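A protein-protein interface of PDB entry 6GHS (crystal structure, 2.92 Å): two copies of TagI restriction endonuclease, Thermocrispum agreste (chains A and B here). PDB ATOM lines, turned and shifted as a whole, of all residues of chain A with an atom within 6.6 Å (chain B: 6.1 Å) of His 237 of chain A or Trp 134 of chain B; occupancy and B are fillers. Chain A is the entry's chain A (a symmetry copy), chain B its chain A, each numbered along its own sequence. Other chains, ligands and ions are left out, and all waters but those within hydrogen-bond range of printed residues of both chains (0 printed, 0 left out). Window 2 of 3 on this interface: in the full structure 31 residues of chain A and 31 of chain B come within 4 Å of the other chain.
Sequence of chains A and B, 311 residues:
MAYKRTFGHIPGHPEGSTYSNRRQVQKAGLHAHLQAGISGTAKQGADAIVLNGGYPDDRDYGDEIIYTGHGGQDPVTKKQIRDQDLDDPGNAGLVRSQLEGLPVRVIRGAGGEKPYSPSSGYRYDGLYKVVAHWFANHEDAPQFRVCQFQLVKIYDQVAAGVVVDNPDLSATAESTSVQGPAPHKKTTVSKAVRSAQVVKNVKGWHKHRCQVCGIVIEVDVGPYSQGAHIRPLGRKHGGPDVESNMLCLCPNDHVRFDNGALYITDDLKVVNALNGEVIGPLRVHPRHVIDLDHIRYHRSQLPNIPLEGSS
The backbone carbonyl oxygen (O) of Trp 134 of chain B is in hydrogen-bond range of the backbone NH (N) of Gln 148 of chain B (2.7 Å). The backbone carbonyl oxygen (O) of His 237 of chain A sits at hydrogen-bond distance from the guanidinium group (NH2) of Arg 231 of chain A (2.9 Å). The side-chain hydroxyl of Tyr 297 of chain A lies within hydrogen-bond range of a ring nitrogen (ND1) of His 237 of chain A (2.6 Å).
Along chain A the printed residues that touch a printed residue of chain B span positions 236 to 302. Hydrophobic or aromatic side chains of chain B that line the printed part of chain A: Trp 134 and Phe 135. Among the printed residues, 7 pairs touch across the chains. Among the printed residues, no Asp or Glu carboxylate lies within 4 Å of a Lys or Arg side-chain nitrogen of the other chain.
The side-chain amino group of Lys 236 of chain A is in hydrogen-bond range of the side-chain amide oxygen of Gln 148 of chain B (3.1 Å). The backbone NH (N) of Phe 135 of chain B is in hydrogen-bond range of the backbone carbonyl oxygen (O) of Gln 301 of chain A, at 3.1 Å.
Among the printed residues, pairs that only touch across the chains: His 237 of chain A with Trp 134 of chain B (3.5 Å), Leu 302 of chain A with Phe 135 of chain B (3.7 Å), Ser 300 of chain A with Phe 135 of chain B (3.7 Å), Lys 236 of chain A with Trp 134 of chain B (3.8 Å) and Gln 301 of chain A with Trp 134 of chain B (3.9 Å).
His 237 of chain A touches just one residue of chain B: Trp 134. Of the printed residues of chain B, Ser 300 of chain A touches Phe 135. Printed residues of chain B within 4 Å of Gln 301 of chain A: Trp 134 (3.9 Å) and Phe 135 (3.1 Å). Of the printed residues of chain B, Leu 302 of chain A touches Phe 135 (3.7 Å). Of chain A, only Lys 236 (3.8 Å), His 237 (3.5 Å) and Gln 301 (3.9 Å) come within 4 Å of Trp 134 of chain B.
No position is printed for both chains. Of the 7 pairs that touch across the chains among the printed residues, none has its exchanged pair printed and touching as well.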
ATOM      1  N   ARG A 231      13.226 -12.828   2.920  1.00  0.00           N
ATOM      2  CA  ARG A 231      13.450 -14.249   3.190  1.00  0.00           C
ATOM      3  C   ARG A 231      14.817 -14.408   3.844  1.00  0.00           C
ATOM      4  O   ARG A 231      15.826 -14.153   3.188  1.00  0.00           O
ATOM      5  CB  ARG A 231      13.418 -15.056   1.905  1.00  0.00           C
ATOM      6  CG  ARG A 231      13.748 -16.524   2.099  1.00  0.00           C
ATOM      7  CD  ARG A 231      13.745 -17.253   0.777  1.00  0.00           C
ATOM      8  NE  ARG A 231      13.854 -18.689   0.979  1.00  0.00           N
ATOM      9  CZ  ARG A 231      13.629 -19.607   0.045  1.00  0.00           C
ATOM     10  NH1 ARG A 231      13.287 -19.254  -1.194  1.00  0.00           N
ATOM     11  NH2 ARG A 231      13.745 -20.895   0.359  1.00  0.00           N
ATOM     12  N   PRO A 232      14.863 -14.862   5.114  1.00  0.00           N
ATOM     13  CA  PRO A 232      16.135 -14.802   5.854  1.00  0.00           C
ATOM     14  C   PRO A 232      17.268 -15.595   5.217  1.00  0.00           C
ATOM     15  O   PRO A 232      17.026 -16.518   4.443  1.00  0.00           O
ATOM     16  CB  PRO A 232      15.786 -15.380   7.233  1.00  0.00           C
ATOM     17  CG  PRO A 232      14.307 -15.351   7.314  1.00  0.00           C
ATOM     18  CD  PRO A 232      13.804 -15.490   5.916  1.00  0.00           C
ATOM     19  N   LEU A 233      18.492 -15.217   5.555  1.00  0.00           N
ATOM     20  CA  LEU A 233      19.676 -15.876   5.030  1.00  0.00           C
ATOM     21  C   LEU A 233      19.967 -17.140   5.834  1.00  0.00           C
ATOM     22  O   LEU A 233      19.426 -17.318   6.926  1.00  0.00           O
ATOM     23  CB  LEU A 233      20.872 -14.924   5.099  1.00  0.00           C
ATOM     24  CG  LEU A 233      20.728 -13.545   4.446  1.00  0.00           C
ATOM     25  CD1 LEU A 233      21.983 -12.723   4.675  1.00  0.00           C
ATOM     26  CD2 LEU A 233      20.442 -13.677   2.954  1.00  0.00           C
ATOM     27  N   GLY A 234      20.804 -18.019   5.285  1.00  0.00           N
ATOM     28  CA  GLY A 234      21.376 -19.134   6.046  1.00  0.00           C
ATOM     29  C   GLY A 234      20.837 -20.511   5.728  1.00  0.00           C
ATOM     30  O   GLY A 234      20.036 -20.685   4.808  1.00  0.00           O
ATOM     31  N   ARG A 235      21.284 -21.482   6.525  1.00  0.00           N
ATOM     32  CA  ARG A 235      21.092 -22.917   6.239  1.00  0.00           C
ATOM     33  C   ARG A 235      19.651 -23.347   6.060  1.00  0.00           C
ATOM     34  O   ARG A 235      19.346 -24.043   5.102  1.00  0.00           O
ATOM     35  CB  ARG A 235      21.727 -23.793   7.327  1.00  0.00           C
ATOM     36  CG  ARG A 235      23.163 -24.192   7.039  1.00  0.00           C
ATOM     37  CD  ARG A 235      23.798 -24.814   8.269  1.00  0.00           C
ATOM     38  NE  ARG A 235      25.250 -24.930   8.136  1.00  0.00           N
ATOM     39  CZ  ARG A 235      26.154 -24.615   9.072  1.00  0.00           C
ATOM     40  NH1 ARG A 235      25.801 -24.119  10.263  1.00  0.00           N
ATOM     41  NH2 ARG A 235      27.451 -24.783   8.803  1.00  0.00           N
ATOM     42  N   LYS A 236      18.775 -22.946   6.976  1.00  0.00           N
ATOM     43  CA  LYS A 236      17.365 -23.365   6.929  1.00  0.00           C
ATOM     44  C   LYS A 236      16.595 -22.734   5.750  1.00  0.00           C
ATOM     45  O   LYS A 236      15.998 -23.446   4.916  1.00  0.00           O
ATOM     46  CB  LYS A 236      16.668 -23.072   8.276  1.00  0.00           C
ATOM     47  CG  LYS A 236      15.150 -23.265   8.317  1.00  0.00           C
ATOM     48  CD  LYS A 236      14.692 -24.711   8.142  1.00  0.00           C
ATOM     49  CE  LYS A 236      13.222 -24.788   7.725  1.00  0.00           C
ATOM     50  NZ  LYS A 236      12.438 -25.787   8.509  1.00  0.00           N
ATOM     51  N   HIS A 237      16.628 -21.404   5.684  1.00  0.00           N
ATOM     52  CA  HIS A 237      15.783 -20.649   4.760  1.00  0.00           C
ATOM     53  C   HIS A 237      16.436 -20.382   3.393  1.00  0.00           C
ATOM     54  O   HIS A 237      15.745 -20.376   2.372  1.00  0.00           O
ATOM     55  CB  HIS A 237      15.347 -19.341   5.419  1.00  0.00           C
ATOM     56  CG  HIS A 237      14.589 -19.526   6.705  1.00  0.00           C
ATOM     57  ND1 HIS A 237      13.296 -20.008   6.747  1.00  0.00           N
ATOM     58  CD2 HIS A 237      14.934 -19.268   7.990  1.00  0.00           C
ATOM     59  CE1 HIS A 237      12.887 -20.052   8.001  1.00  0.00           C
ATOM     60  NE2 HIS A 237      13.859 -19.605   8.775  1.00  0.00           N
ATOM     61  N   GLY A 238      17.752 -20.157   3.380  1.00  0.00           N
ATOM     62  CA  GLY A 238      18.524 -20.021   2.135  1.00  0.00           C
ATOM     63  C   GLY A 238      18.067 -18.873   1.257  1.00  0.00           C
ATOM     64  O   GLY A 238      17.840 -19.039   0.058  1.00  0.00           O
ATOM     65  N   GLY A 239      17.910 -17.709   1.871  1.00  0.00           N
ATOM     66  CA  GLY A 239      17.555 -16.498   1.151  1.00  0.00           C
ATOM     67  C   GLY A 239      18.781 -15.934   0.462  1.00  0.00           C
ATOM     68  O   GLY A 239      19.888 -16.037   0.983  1.00  0.00           O
ATOM     69  N   PRO A 240      18.596 -15.345  -0.721  1.00  0.00           N
ATOM     70  CA  PRO A 240      19.720 -14.707  -1.369  1.00  0.00           C
ATOM     71  C   PRO A 240      19.991 -13.351  -0.736  1.00  0.00           C
ATOM     72  O   PRO A 240      19.055 -12.683  -0.263  1.00  0.00           O
ATOM     73  CB  PRO A 240      19.221 -14.534  -2.802  1.00  0.00           C
ATOM     74  CG  PRO A 240      17.755 -14.291  -2.644  1.00  0.00           C
ATOM     75  CD  PRO A 240      17.357 -15.198  -1.510  1.00  0.00           C
ATOM     76  N   TYR A 297       7.227 -16.210   0.952  1.00  0.00           N
ATOM     77  CA  TYR A 297       7.985 -17.042   1.917  1.00  0.00           C
ATOM     78  C   TYR A 297       7.918 -16.477   3.329  1.00  0.00           C
ATOM     79  O   TYR A 297       7.652 -17.202   4.284  1.00  0.00           O
ATOM     80  CB  TYR A 297       9.459 -17.199   1.498  1.00  0.00           C
ATOM     81  CG  TYR A 297      10.206 -18.235   2.301  1.00  0.00           C
ATOM     82  CD1 TYR A 297      10.672 -17.944   3.588  1.00  0.00           C
ATOM     83  CD2 TYR A 297      10.439 -19.519   1.789  1.00  0.00           C
ATOM     84  CE1 TYR A 297      11.349 -18.894   4.349  1.00  0.00           C
ATOM     85  CE2 TYR A 297      11.118 -20.484   2.538  1.00  0.00           C
ATOM     86  CZ  TYR A 297      11.574 -20.165   3.821  1.00  0.00           C
ATOM     87  OH  TYR A 297      12.251 -21.096   4.582  1.00  0.00           O
ATOM     88  N   SER A 300       4.665 -16.862   4.911  1.00  0.00           N
ATOM     89  CA  SER A 300       4.493 -18.256   5.273  1.00  0.00           C
ATOM     90  C   SER A 300       5.248 -18.708   6.521  1.00  0.00           C
ATOM     91  O   SER A 300       5.203 -19.888   6.846  1.00  0.00           O
ATOM     92  CB  SER A 300       4.850 -19.149   4.066  1.00  0.00           C
ATOM     93  OG  SER A 300       3.830 -19.075   3.073  1.00  0.00           O
ATOM     94  N   GLN A 301       5.942 -17.798   7.212  1.00  0.00           N
ATOM     95  CA  GLN A 301       6.530 -18.073   8.542  1.00  0.00           C
ATOM     96  C   GLN A 301       5.573 -17.776   9.698  1.00  0.00           C
ATOM     97  O   GLN A 301       5.913 -18.049  10.848  1.00  0.00           O
ATOM     98  CB  GLN A 301       7.783 -17.231   8.784  1.00  0.00           C
ATOM     99  CG  GLN A 301       8.935 -17.409   7.814  1.00  0.00           C
ATOM    100  CD  GLN A 301      10.085 -16.481   8.169  1.00  0.00           C
ATOM    101  OE1 GLN A 301       9.924 -15.255   8.158  1.00  0.00           O
ATOM    102  NE2 GLN A 301      11.238 -17.056   8.527  1.00  0.00           N
ATOM    103  N   LEU A 302       4.408 -17.194   9.414  1.00  0.00           N
ATOM    104  CA  LEU A 302       3.438 -16.888  10.457  1.00  0.00           C
ATOM    105  C   LEU A 302       2.733 -18.162  10.937  1.00  0.00           C
ATOM    106  O   LEU A 302       2.777 -19.169  10.246  1.00  0.00           O
ATOM    107  CB  LEU A 302       2.416 -15.880   9.936  1.00  0.00           C
ATOM    108  CG  LEU A 302       2.992 -14.512   9.599  1.00  0.00           C
ATOM    109  CD1 LEU A 302       1.999 -13.728   8.766  1.00  0.00           C
ATOM    110  CD2 LEU A 302       3.357 -13.746  10.864  1.00  0.00           C
ATOM    111  N   ILE B  66      18.617 -25.921  14.646  1.00  0.00           N
ATOM    112  CA  ILE B  66      17.210 -25.677  14.385  1.00  0.00           C
ATOM    113  C   ILE B  66      16.451 -26.533  15.391  1.00  0.00           C
ATOM    114  O   ILE B  66      16.358 -27.746  15.210  1.00  0.00           O
ATOM    115  CB  ILE B  66      16.801 -26.049  12.937  1.00  0.00           C
ATOM    116  CG1 ILE B  66      17.786 -25.479  11.920  1.00  0.00           C
ATOM    117  CG2 ILE B  66      15.402 -25.544  12.628  1.00  0.00           C
ATOM    118  CD1 ILE B  66      18.149 -24.027  12.144  1.00  0.00           C
ATOM    119  N   ALA B 132      16.421 -16.351  15.738  1.00  0.00           N
ATOM    120  CA  ALA B 132      15.142 -16.147  15.060  1.00  0.00           C
ATOM    121  C   ALA B 132      14.185 -17.262  15.379  1.00  0.00           C
ATOM    122  O   ALA B 132      14.599 -18.299  15.892  1.00  0.00           O
ATOM    123  CB  ALA B 132      15.354 -16.075  13.558  1.00  0.00           C
ATOM    124  N   HIS B 133      12.909 -17.040  15.070  1.00  0.00           N
ATOM    125  CA  HIS B 133      11.892 -18.080  15.192  1.00  0.00           C
ATOM    126  C   HIS B 133      10.849 -17.991  14.090  1.00  0.00           C
ATOM    127  O   HIS B 133      10.625 -16.938  13.522  1.00  0.00           O
ATOM    128  CB  HIS B 133      11.207 -17.990  16.543  1.00  0.00           C
ATOM    129  CG  HIS B 133      10.364 -16.771  16.698  1.00  0.00           C
ATOM    130  ND1 HIS B 133      10.813 -15.636  17.335  1.00  0.00           N
ATOM    131  CD2 HIS B 133       9.105 -16.497  16.281  1.00  0.00           C
ATOM    132  CE1 HIS B 133       9.860 -14.719  17.318  1.00  0.00           C
ATOM    133  NE2 HIS B 133       8.812 -15.218  16.687  1.00  0.00           N
ATOM    134  N   TRP B 134      10.203 -19.107  13.804  1.00  0.00           N
ATOM    135  CA  TRP B 134       9.190 -19.158  12.760  1.00  0.00           C
ATOM    136  C   TRP B 134       8.291 -20.353  12.973  1.00  0.00           C
ATOM    137  O   TRP B 134       8.508 -21.148  13.889  1.00  0.00           O
ATOM    138  CB  TRP B 134       9.858 -19.273  11.389  1.00  0.00           C
ATOM    139  CG  TRP B 134      10.733 -20.464  11.304  1.00  0.00           C
ATOM    140  CD1 TRP B 134      10.382 -21.723  10.906  1.00  0.00           C
ATOM    141  CD2 TRP B 134      12.108 -20.527  11.670  1.00  0.00           C
ATOM    142  NE1 TRP B 134      11.464 -22.563  10.988  1.00  0.00           N
ATOM    143  CE2 TRP B 134      12.537 -21.853  11.453  1.00  0.00           C
ATOM    144  CE3 TRP B 134      13.026 -19.584  12.156  1.00  0.00           C
ATOM    145  CZ2 TRP B 134      13.838 -22.263  11.704  1.00  0.00           C
ATOM    146  CZ3 TRP B 134      14.323 -19.992  12.408  1.00  0.00           C
ATOM    147  CH2 TRP B 134      14.719 -21.323  12.183  1.00  0.00           C
ATOM    148  N   PHE B 135       7.283 -20.468  12.112  1.00  0.00           N
ATOM    149  CA  PHE B 135       6.451 -21.661  12.028  1.00  0.00           C
ATOM    150  C   PHE B 135       6.666 -22.337  10.696  1.00  0.00           C
ATOM    151  O   PHE B 135       6.883 -21.666   9.679  1.00  0.00           O
ATOM    152  CB  PHE B 135       4.990 -21.313  12.234  1.00  0.00           C
ATOM    153  CG  PHE B 135       4.680 -20.962  13.646  1.00  0.00           C
ATOM    154  CD1 PHE B 135       5.034 -19.719  14.154  1.00  0.00           C
ATOM    155  CD2 PHE B 135       4.089 -21.884  14.489  1.00  0.00           C
ATOM    156  CE1 PHE B 135       4.772 -19.391  15.474  1.00  0.00           C
ATOM    157  CE2 PHE B 135       3.823 -21.563  15.806  1.00  0.00           C
ATOM    158  CZ  PHE B 135       4.165 -20.315  16.301  1.00  0.00           C
ATOM    159  N   ALA B 136       6.648 -23.667  10.723  1.00  0.00           N
ATOM    160  CA  ALA B 136       6.746 -24.479   9.511  1.00  0.00           C
ATOM    161  C   ALA B 136       5.783 -25.649   9.631  1.00  0.00           C
ATOM    162  O   ALA B 136       5.111 -25.800  10.651  1.00  0.00           O
ATOM    163  CB  ALA B 136       8.176 -24.966   9.305  1.00  0.00           C
ATOM    164  N   VAL B 146       4.358 -26.415  13.295  1.00  0.00           N
ATOM    165  CA  VAL B 146       5.205 -26.392  14.485  1.00  0.00           C
ATOM    166  C   VAL B 146       6.006 -25.102  14.536  1.00  0.00           C
ATOM    167  O   VAL B 146       6.274 -24.476  13.507  1.00  0.00           O
ATOM    168  CB  VAL B 146       6.186 -27.581  14.550  1.00  0.00           C
ATOM    169  CG1 VAL B 146       5.425 -28.861  14.842  1.00  0.00           C
ATOM    170  CG2 VAL B 146       7.022 -27.711  13.269  1.00  0.00           C
ATOM    171  N   CYS B 147       6.395 -24.748  15.752  1.00  0.00           N
ATOM    172  CA  CYS B 147       7.230 -23.603  16.028  1.00  0.00           C
ATOM    173  C   CYS B 147       8.698 -24.011  15.955  1.00  0.00           C
ATOM    174  O   CYS B 147       9.042 -25.086  16.403  1.00  0.00           O
ATOM    175  CB  CYS B 147       6.906 -23.117  17.429  1.00  0.00           C
ATOM    176  SG  CYS B 147       7.561 -21.486  17.741  1.00  0.00           S
ATOM    177  N   GLN B 148       9.563 -23.164  15.413  1.00  0.00           N
ATOM    178  CA  GLN B 148      10.991 -23.492  15.321  1.00  0.00           C
ATOM    179  C   GLN B 148      11.901 -22.321  15.659  1.00  0.00           C
ATOM    180  O   GLN B 148      11.539 -21.167  15.487  1.00  0.00           O
ATOM    181  CB  GLN B 148      11.330 -24.017  13.931  1.00  0.00           C
ATOM    182  CG  GLN B 148      11.171 -25.517  13.799  1.00  0.00           C
ATOM    183  CD  GLN B 148      11.557 -26.032  12.426  1.00  0.00           C
ATOM    184  OE1 GLN B 148      11.294 -25.392  11.402  1.00  0.00           O
ATOM    185  NE2 GLN B 148      12.184 -27.200  12.396  1.00  0.00           N
ATOM    186  N   PHE B 149      13.093 -22.642  16.136  1.00  0.00           N
ATOM    187  CA  PHE B 149      14.040 -21.647  16.607  1.00  0.00           C
ATOM    188  C   PHE B 149      15.395 -21.906  15.966  1.00  0.00           C
ATOM    189  O   PHE B 149      15.736 -23.046  15.664  1.00  0.00           O
ATOM    190  CB  PHE B 149      14.140 -21.695  18.139  1.00  0.00           C
ATOM    191  CG  PHE B 149      12.818 -21.518  18.830  1.00  0.00           C
ATOM    192  CD1 PHE B 149      11.982 -22.603  19.041  1.00  0.00           C
ATOM    193  CD2 PHE B 149      12.392 -20.255  19.246  1.00  0.00           C
ATOM    194  CE1 PHE B 149      10.756 -22.432  19.661  1.00  0.00           C
ATOM    195  CE2 PHE B 149      11.163 -20.079  19.862  1.00  0.00           C
ATOM    196  CZ  PHE B 149      10.349 -21.168  20.075  1.00  0.00           C
ATOM    197  N   GLN B 150      16.147 -20.832  15.746  1.00  0.00           N
ATOM    198  CA  GLN B 150      17.533 -20.921  15.332  1.00  0.00           C
ATOM    199  C   GLN B 150      18.445 -20.534  16.503  1.00  0.00           C
ATOM    200  O   GLN B 150      18.337 -19.423  17.036  1.00  0.00           O
ATOM    201  CB  GLN B 150      17.770 -19.998  14.153  1.00  0.00           C
ATOM    202  CG  GLN B 150      19.086 -20.256  13.438  1.00  0.00           C
ATOM    203  CD  GLN B 150      19.356 -19.243  12.350  1.00  0.00           C
ATOM    204  OE1 GLN B 150      18.921 -18.093  12.433  1.00  0.00           O
ATOM    205  NE2 GLN B 150      20.080 -19.664  11.321  1.00  0.00           N
